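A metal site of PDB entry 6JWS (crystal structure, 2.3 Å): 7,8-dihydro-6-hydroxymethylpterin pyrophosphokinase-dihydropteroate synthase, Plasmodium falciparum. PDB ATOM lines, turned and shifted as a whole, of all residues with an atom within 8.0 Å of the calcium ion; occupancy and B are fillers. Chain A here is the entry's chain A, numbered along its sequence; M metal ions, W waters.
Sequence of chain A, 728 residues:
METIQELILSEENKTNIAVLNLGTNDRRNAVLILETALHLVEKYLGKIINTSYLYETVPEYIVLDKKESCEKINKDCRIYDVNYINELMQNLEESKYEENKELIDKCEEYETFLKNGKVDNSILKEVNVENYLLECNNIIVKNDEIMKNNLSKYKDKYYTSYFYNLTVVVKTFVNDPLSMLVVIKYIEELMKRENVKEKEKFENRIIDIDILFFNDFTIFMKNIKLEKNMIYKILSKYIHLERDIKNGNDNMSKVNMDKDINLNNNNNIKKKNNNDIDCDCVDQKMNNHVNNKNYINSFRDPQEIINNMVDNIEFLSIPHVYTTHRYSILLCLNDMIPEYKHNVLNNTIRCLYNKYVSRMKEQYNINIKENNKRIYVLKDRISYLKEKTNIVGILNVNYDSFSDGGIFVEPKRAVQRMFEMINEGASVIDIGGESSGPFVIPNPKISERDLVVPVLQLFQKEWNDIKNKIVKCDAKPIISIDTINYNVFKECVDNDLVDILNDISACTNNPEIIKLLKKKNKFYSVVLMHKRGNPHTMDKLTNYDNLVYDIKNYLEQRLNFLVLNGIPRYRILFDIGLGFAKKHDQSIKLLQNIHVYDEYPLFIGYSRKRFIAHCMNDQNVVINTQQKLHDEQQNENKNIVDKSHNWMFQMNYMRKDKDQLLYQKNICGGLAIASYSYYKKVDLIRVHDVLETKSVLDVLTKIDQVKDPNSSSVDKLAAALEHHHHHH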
ATOM      1  N   LEU A  38       0.100 -23.769  25.927  1.00  0.00           N
ATOM      2  CA  LEU A  38      -0.176 -23.128  24.643  1.00  0.00           C
ATOM      3  C   LEU A  38       0.905 -23.480  23.602  1.00  0.00           C
ATOM      4  O   LEU A  38       0.585 -23.843  22.471  1.00  0.00           O
ATOM      5  CB  LEU A  38      -0.217 -21.608  24.809  1.00  0.00           C
ATOM      6  CG  LEU A  38      -1.441 -21.028  25.505  1.00  0.00           C
ATOM      7  CD1 LEU A  38      -1.349 -19.519  25.490  1.00  0.00           C
ATOM      8  CD2 LEU A  38      -2.703 -21.484  24.809  1.00  0.00           C
ATOM      9  N   HIS A  39       2.166 -23.376  24.003  1.00  0.00           N
ATOM     10  CA  HIS A  39       3.267 -23.718  23.122  1.00  0.00           C
ATOM     11  C   HIS A  39       3.125 -25.147  22.623  1.00  0.00           C
ATOM     12  O   HIS A  39       3.339 -25.401  21.432  1.00  0.00           O
ATOM     13  CB  HIS A  39       4.613 -23.510  23.826  1.00  0.00           C
ATOM     14  CG  HIS A  39       4.980 -22.065  23.971  1.00  0.00           C
ATOM     15  ND1 HIS A  39       5.281 -21.508  25.207  1.00  0.00           N
ATOM     16  CD2 HIS A  39       5.070 -21.072  23.073  1.00  0.00           C
ATOM     17  CE1 HIS A  39       5.560 -20.234  25.051  1.00  0.00           C
ATOM     18  NE2 HIS A  39       5.448 -19.942  23.748  1.00  0.00           N
ATOM     19  N   LEU A  40       2.720 -26.060  23.526  1.00  0.00           N
ATOM     20  CA  LEU A  40       2.677 -27.477  23.189  1.00  0.00           C
ATOM     21  C   LEU A  40       1.460 -27.762  22.316  1.00  0.00           C
ATOM     22  O   LEU A  40       1.515 -28.664  21.488  1.00  0.00           O
ATOM     23  CB  LEU A  40       2.693 -28.334  24.467  1.00  0.00           C
ATOM     24  CG  LEU A  40       4.021 -28.268  25.241  1.00  0.00           C
ATOM     25  CD1 LEU A  40       3.926 -29.001  26.579  1.00  0.00           C
ATOM     26  CD2 LEU A  40       5.180 -28.768  24.390  1.00  0.00           C
ATOM     27  N   VAL A  41       0.405 -26.969  22.504  1.00  0.00           N
ATOM     28  CA  VAL A  41      -0.760 -27.032  21.631  1.00  0.00           C
ATOM     29  C   VAL A  41      -0.375 -26.577  20.224  1.00  0.00           C
ATOM     30  O   VAL A  41      -0.799 -27.185  19.245  1.00  0.00           O
ATOM     31  CB  VAL A  41      -1.938 -26.191  22.148  1.00  0.00           C
ATOM     32  CG1 VAL A  41      -3.022 -26.080  21.085  1.00  0.00           C
ATOM     33  CG2 VAL A  41      -2.504 -26.755  23.444  1.00  0.00           C
ATOM     34  N   GLU A  42       0.380 -25.467  20.131  1.00  0.00           N
ATOM     35  CA  GLU A  42       0.769 -24.917  18.837  1.00  0.00           C
ATOM     36  C   GLU A  42       1.692 -25.909  18.138  1.00  0.00           C
ATOM     37  O   GLU A  42       1.667 -26.031  16.919  1.00  0.00           O
ATOM     38  CB  GLU A  42       1.550 -23.612  19.018  1.00  0.00           C
ATOM     39  CG  GLU A  42       0.749 -22.354  18.738  1.00  0.00           C
ATOM     40  CD  GLU A  42       0.316 -22.059  17.304  1.00  0.00           C
ATOM     41  OE1 GLU A  42       0.754 -22.786  16.350  1.00  0.00           O
ATOM     42  OE2 GLU A  42      -0.487 -21.117  17.134  1.00  0.00           O
ATOM     43  N   LYS A  43       2.530 -26.590  18.936  1.00  0.00           N
ATOM     44  CA  LYS A  43       3.501 -27.528  18.384  1.00  0.00           C
ATOM     45  C   LYS A  43       2.823 -28.816  17.920  1.00  0.00           C
ATOM     46  O   LYS A  43       3.134 -29.308  16.843  1.00  0.00           O
ATOM     47  CB  LYS A  43       4.600 -27.815  19.413  1.00  0.00           C
ATOM     48  CG  LYS A  43       5.744 -28.716  18.960  1.00  0.00           C
ATOM     49  CD  LYS A  43       6.823 -28.850  20.042  1.00  0.00           C
ATOM     50  CE  LYS A  43       8.073 -29.602  19.606  1.00  0.00           C
ATOM     51  NZ  LYS A  43       8.835 -28.907  18.538  1.00  0.00           N
ATOM     52  N   TYR A  44       1.894 -29.335  18.741  1.00  0.00           N
ATOM     53  CA  TYR A  44       1.441 -30.706  18.611  1.00  0.00           C
ATOM     54  C   TYR A  44       0.030 -30.817  18.013  1.00  0.00           C
ATOM     55  O   TYR A  44      -0.327 -31.909  17.530  1.00  0.00           O
ATOM     56  CB  TYR A  44       1.598 -31.473  19.927  1.00  0.00           C
ATOM     57  CG  TYR A  44       3.006 -31.812  20.326  1.00  0.00           C
ATOM     58  CD1 TYR A  44       3.939 -32.248  19.390  1.00  0.00           C
ATOM     59  CD2 TYR A  44       3.406 -31.726  21.661  1.00  0.00           C
ATOM     60  CE1 TYR A  44       5.233 -32.553  19.767  1.00  0.00           C
ATOM     61  CE2 TYR A  44       4.707 -32.027  22.050  1.00  0.00           C
ATOM     62  CZ  TYR A  44       5.617 -32.454  21.097  1.00  0.00           C
ATOM     63  OH  TYR A  44       6.894 -32.767  21.470  1.00  0.00           O
ATOM     64  N   LEU A  45      -0.773 -29.738  18.027  1.00  0.00           N
ATOM     65  CA  LEU A  45      -2.187 -29.868  17.688  1.00  0.00           C
ATOM     66  C   LEU A  45      -2.610 -29.052  16.463  1.00  0.00           C
ATOM     67  O   LEU A  45      -3.599 -29.367  15.820  1.00  0.00           O
ATOM     68  CB  LEU A  45      -3.064 -29.542  18.911  1.00  0.00           C
ATOM     69  CG  LEU A  45      -2.955 -30.542  20.062  1.00  0.00           C
ATOM     70  CD1 LEU A  45      -3.770 -30.092  21.259  1.00  0.00           C
ATOM     71  CD2 LEU A  45      -3.427 -31.917  19.584  1.00  0.00           C
ATOM     72  N   GLY A  46      -1.933 -27.938  16.183  1.00  0.00           N
ATOM     73  CA  GLY A  46      -2.262 -27.151  15.006  1.00  0.00           C
ATOM     74  C   GLY A  46      -1.980 -25.675  15.242  1.00  0.00           C
ATOM     75  O   GLY A  46      -0.929 -25.327  15.766  1.00  0.00           O
ATOM     76  N   LYS A  47      -2.937 -24.807  14.885  1.00  0.00           N
ATOM     77  CA  LYS A  47      -2.713 -23.381  14.960  1.00  0.00           C
ATOM     78  C   LYS A  47      -3.730 -22.727  15.899  1.00  0.00           C
ATOM     79  O   LYS A  47      -4.933 -22.875  15.702  1.00  0.00           O
ATOM     80  CB  LYS A  47      -2.769 -22.770  13.551  1.00  0.00           C
ATOM     81  CG  LYS A  47      -2.507 -21.265  13.511  1.00  0.00           C
ATOM     82  CD  LYS A  47      -2.658 -20.638  12.127  1.00  0.00           C
ATOM     83  CE  LYS A  47      -2.269 -19.169  12.061  1.00  0.00           C
ATOM     84  NZ  LYS A  47      -1.034 -18.859  12.824  1.00  0.00           N
ATOM     85  N   ILE A  48      -3.221 -21.969  16.888  1.00  0.00           N
ATOM     86  CA  ILE A  48      -4.080 -21.147  17.743  1.00  0.00           C
ATOM     87  C   ILE A  48      -4.526 -19.900  16.970  1.00  0.00           C
ATOM     88  O   ILE A  48      -3.698 -19.137  16.469  1.00  0.00           O
ATOM     89  CB  ILE A  48      -3.334 -20.790  19.044  1.00  0.00           C
ATOM     90  CG1 ILE A  48      -2.933 -22.044  19.825  1.00  0.00           C
ATOM     91  CG2 ILE A  48      -4.145 -19.826  19.889  1.00  0.00           C
ATOM     92  CD1 ILE A  48      -2.128 -21.765  21.092  1.00  0.00           C
ATOM     93  N   SER A  95       7.082 -32.507  16.128  1.00  0.00           N
ATOM     94  CA  SER A  95       5.819 -32.823  15.482  1.00  0.00           C
ATOM     95  C   SER A  95       6.101 -33.332  14.076  1.00  0.00           C
ATOM     96  O   SER A  95       7.146 -33.032  13.520  1.00  0.00           O
ATOM     97  CB  SER A  95       4.947 -31.587  15.422  1.00  0.00           C
ATOM     98  OG  SER A  95       3.807 -31.806  14.610  1.00  0.00           O
ATOM     99  N   TYR A  97       3.897 -32.492  11.814  1.00  0.00           N
ATOM    100  CA  TYR A  97       3.185 -31.510  11.025  1.00  0.00           C
ATOM    101  C   TYR A  97       3.925 -30.171  11.038  1.00  0.00           C
ATOM    102  O   TYR A  97       4.558 -29.818  12.048  1.00  0.00           O
ATOM    103  CB  TYR A  97       1.719 -31.374  11.465  1.00  0.00           C
ATOM    104  CG  TYR A  97       0.859 -32.536  11.062  1.00  0.00           C
ATOM    105  CD1 TYR A  97       0.966 -33.752  11.719  1.00  0.00           C
ATOM    106  CD2 TYR A  97      -0.054 -32.433  10.017  1.00  0.00           C
ATOM    107  CE1 TYR A  97       0.217 -34.850  11.345  1.00  0.00           C
ATOM    108  CE2 TYR A  97      -0.822 -33.530   9.627  1.00  0.00           C
ATOM    109  CZ  TYR A  97      -0.683 -34.730  10.303  1.00  0.00           C
ATOM    110  OH  TYR A  97      -1.409 -35.849  10.009  1.00  0.00           O
ATOM    111  N   GLU A  98       3.787 -29.420   9.936  1.00  0.00           N
ATOM    112  CA  GLU A  98       4.578 -28.210   9.738  1.00  0.00           C
ATOM    113  C   GLU A  98       3.990 -27.042  10.537  1.00  0.00           C
ATOM    114  O   GLU A  98       2.807 -27.036  10.882  1.00  0.00           O
ATOM    115  CB  GLU A  98       4.826 -27.881   8.264  1.00  0.00           C
ATOM    116  CG  GLU A  98       3.602 -27.853   7.361  1.00  0.00           C
ATOM    117  CD  GLU A  98       3.856 -27.395   5.927  1.00  0.00           C
ATOM    118  OE1 GLU A  98       5.003 -27.550   5.430  1.00  0.00           O
ATOM    119  OE2 GLU A  98       2.895 -26.843   5.306  1.00  0.00           O
ATOM    120  N   GLU A  99       4.853 -26.070  10.841  1.00  0.00           N
ATOM    121  CA  GLU A  99       4.488 -24.852  11.524  1.00  0.00           C
ATOM    122  C   GLU A  99       4.678 -23.643  10.587  1.00  0.00           C
ATOM    123  O   GLU A  99       5.810 -23.207  10.396  1.00  0.00           O
ATOM    124  CB  GLU A  99       5.368 -24.763  12.775  1.00  0.00           C
ATOM    125  CG  GLU A  99       5.061 -23.567  13.662  1.00  0.00           C
ATOM    126  CD  GLU A  99       3.630 -23.614  14.178  1.00  0.00           C
ATOM    127  OE1 GLU A  99       2.697 -23.262  13.392  1.00  0.00           O
ATOM    128  OE2 GLU A  99       3.445 -24.082  15.330  1.00  0.00           O
ATOM    129  N   ASN A 100       3.589 -23.082  10.044  1.00  0.00           N
ATOM    130  CA  ASN A 100       3.622 -21.926   9.148  1.00  0.00           C
ATOM    131  C   ASN A 100       3.369 -20.625   9.902  1.00  0.00           C
ATOM    132  O   ASN A 100       2.365 -20.468  10.585  1.00  0.00           O
ATOM    133  CB  ASN A 100       2.631 -22.073   7.992  1.00  0.00           C
ATOM    134  CG  ASN A 100       2.991 -23.218   7.067  1.00  0.00           C
ATOM    135  OD1 ASN A 100       4.091 -23.291   6.513  1.00  0.00           O
ATOM    136  ND2 ASN A 100       2.071 -24.151   6.902  1.00  0.00           N
ATOM    137  N   LYS A 101       4.263 -19.637   9.768  1.00  0.00           N
ATOM    138  CA  LYS A 101       4.112 -18.428  10.564  1.00  0.00           C
ATOM    139  C   LYS A 101       3.526 -17.258   9.775  1.00  0.00           C
ATOM    140  O   LYS A 101       3.325 -16.194  10.341  1.00  0.00           O
ATOM    141  CB  LYS A 101       5.447 -18.006  11.176  1.00  0.00           C
ATOM    142  CG  LYS A 101       6.026 -18.995  12.178  1.00  0.00           C
ATOM    143  CD  LYS A 101       7.277 -18.467  12.869  1.00  0.00           C
ATOM    144  CE  LYS A 101       7.981 -19.537  13.678  1.00  0.00           C
ATOM    145  NZ  LYS A 101       9.367 -19.152  14.036  1.00  0.00           N
ATOM    146  N   VAL A 170      -8.298 -23.821  18.355  1.00  0.00           N
ATOM    147  CA  VAL A 170      -7.205 -24.434  17.613  1.00  0.00           C
ATOM    148  C   VAL A 170      -7.749 -24.958  16.288  1.00  0.00           C
ATOM    149  O   VAL A 170      -8.683 -25.764  16.283  1.00  0.00           O
ATOM    150  CB  VAL A 170      -6.571 -25.578  18.435  1.00  0.00           C
ATOM    151  CG1 VAL A 170      -5.336 -26.163  17.753  1.00  0.00           C
ATOM    152  CG2 VAL A 170      -6.255 -25.153  19.854  1.00  0.00           C
ATOM    153  N   LYS A 171      -7.145 -24.505  15.181  1.00  0.00           N
ATOM    154  CA  LYS A 171      -7.366 -25.124  13.886  1.00  0.00           C
ATOM    155  C   LYS A 171      -6.429 -26.323  13.849  1.00  0.00           C
ATOM    156  O   LYS A 171      -5.215 -26.137  13.893  1.00  0.00           O
ATOM    157  CB  LYS A 171      -6.990 -24.168  12.756  1.00  0.00           C
ATOM    158  CG  LYS A 171      -7.425 -24.598  11.367  1.00  0.00           C
ATOM    159  CD  LYS A 171      -6.824 -23.837  10.179  1.00  0.00           C
ATOM    160  CE  LYS A 171      -6.529 -22.362  10.367  1.00  0.00           C
ATOM    161  NZ  LYS A 171      -6.743 -21.580   9.108  1.00  0.00           N
ATOM    162  N   PHE A 173      -4.921 -30.297  12.885  1.00  0.00           N
ATOM    163  CA  PHE A 173      -4.708 -31.339  11.896  1.00  0.00           C
ATOM    164  C   PHE A 173      -5.065 -32.718  12.489  1.00  0.00           C
ATOM    165  O   PHE A 173      -4.911 -33.751  11.826  1.00  0.00           O
ATOM    166  CB  PHE A 173      -3.262 -31.306  11.395  1.00  0.00           C
ATOM    167  CG  PHE A 173      -2.228 -31.107  12.468  1.00  0.00           C
ATOM    168  CD1 PHE A 173      -1.889 -32.144  13.341  1.00  0.00           C
ATOM    169  CD2 PHE A 173      -1.577 -29.889  12.604  1.00  0.00           C
ATOM    170  CE1 PHE A 173      -0.934 -31.949  14.330  1.00  0.00           C
ATOM    171  CE2 PHE A 173      -0.615 -29.703  13.585  1.00  0.00           C
ATOM    172  CZ  PHE A 173      -0.302 -30.730  14.451  1.00  0.00           C
ATOM    173  N   LYS A 518       6.350 -14.018  19.280  1.00  0.00           N
ATOM    174  CA  LYS A 518       6.278 -15.421  19.662  1.00  0.00           C
ATOM    175  C   LYS A 518       7.619 -16.106  19.406  1.00  0.00           C
ATOM    176  O   LYS A 518       8.209 -15.907  18.341  1.00  0.00           O
ATOM    177  CB  LYS A 518       5.279 -16.164  18.765  1.00  0.00           C
ATOM    178  CG  LYS A 518       3.824 -15.771  18.954  1.00  0.00           C
ATOM    179  CD  LYS A 518       2.997 -15.893  17.698  1.00  0.00           C
ATOM    180  CE  LYS A 518       2.454 -17.286  17.471  1.00  0.00           C
ATOM    181  NZ  LYS A 518       1.382 -17.272  16.456  1.00  0.00           N
HETATM  182 CA    CA M   1       1.213 -24.699  15.001  1.00  0.00          CA
HETATM  183  O   HOH W   1      -0.082 -24.467  13.057  1.00  0.00           O
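OE2 of Glu 42 sits at hydrogen-bond distance from N of Ile 48, 2.9 Å away.
The backbone NH of Gly 46 sits at hydrogen-bond distance from the backbone carbonyl oxygen of Val 41.
Three residues have an atom within 4 Å of the calcium ion: Glu 42, Gly 46 and Glu 99.
The nearest printed residue that does not touch the calcium ion is Lys 47 (4.1 Å).
The calcium ion is bound by the side-chain carboxylate (OE2) of Glu 99, water W1, the backbone carbonyl oxygen (O) of Gly 46, the backbone carbonyl oxygen (O) of Glu 42, the side-chain carboxylate (OE1) of Glu 42 and the side-chain carboxylate (OE1) of Glu 99.
The calcium ion has six donor atoms within binding distance.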
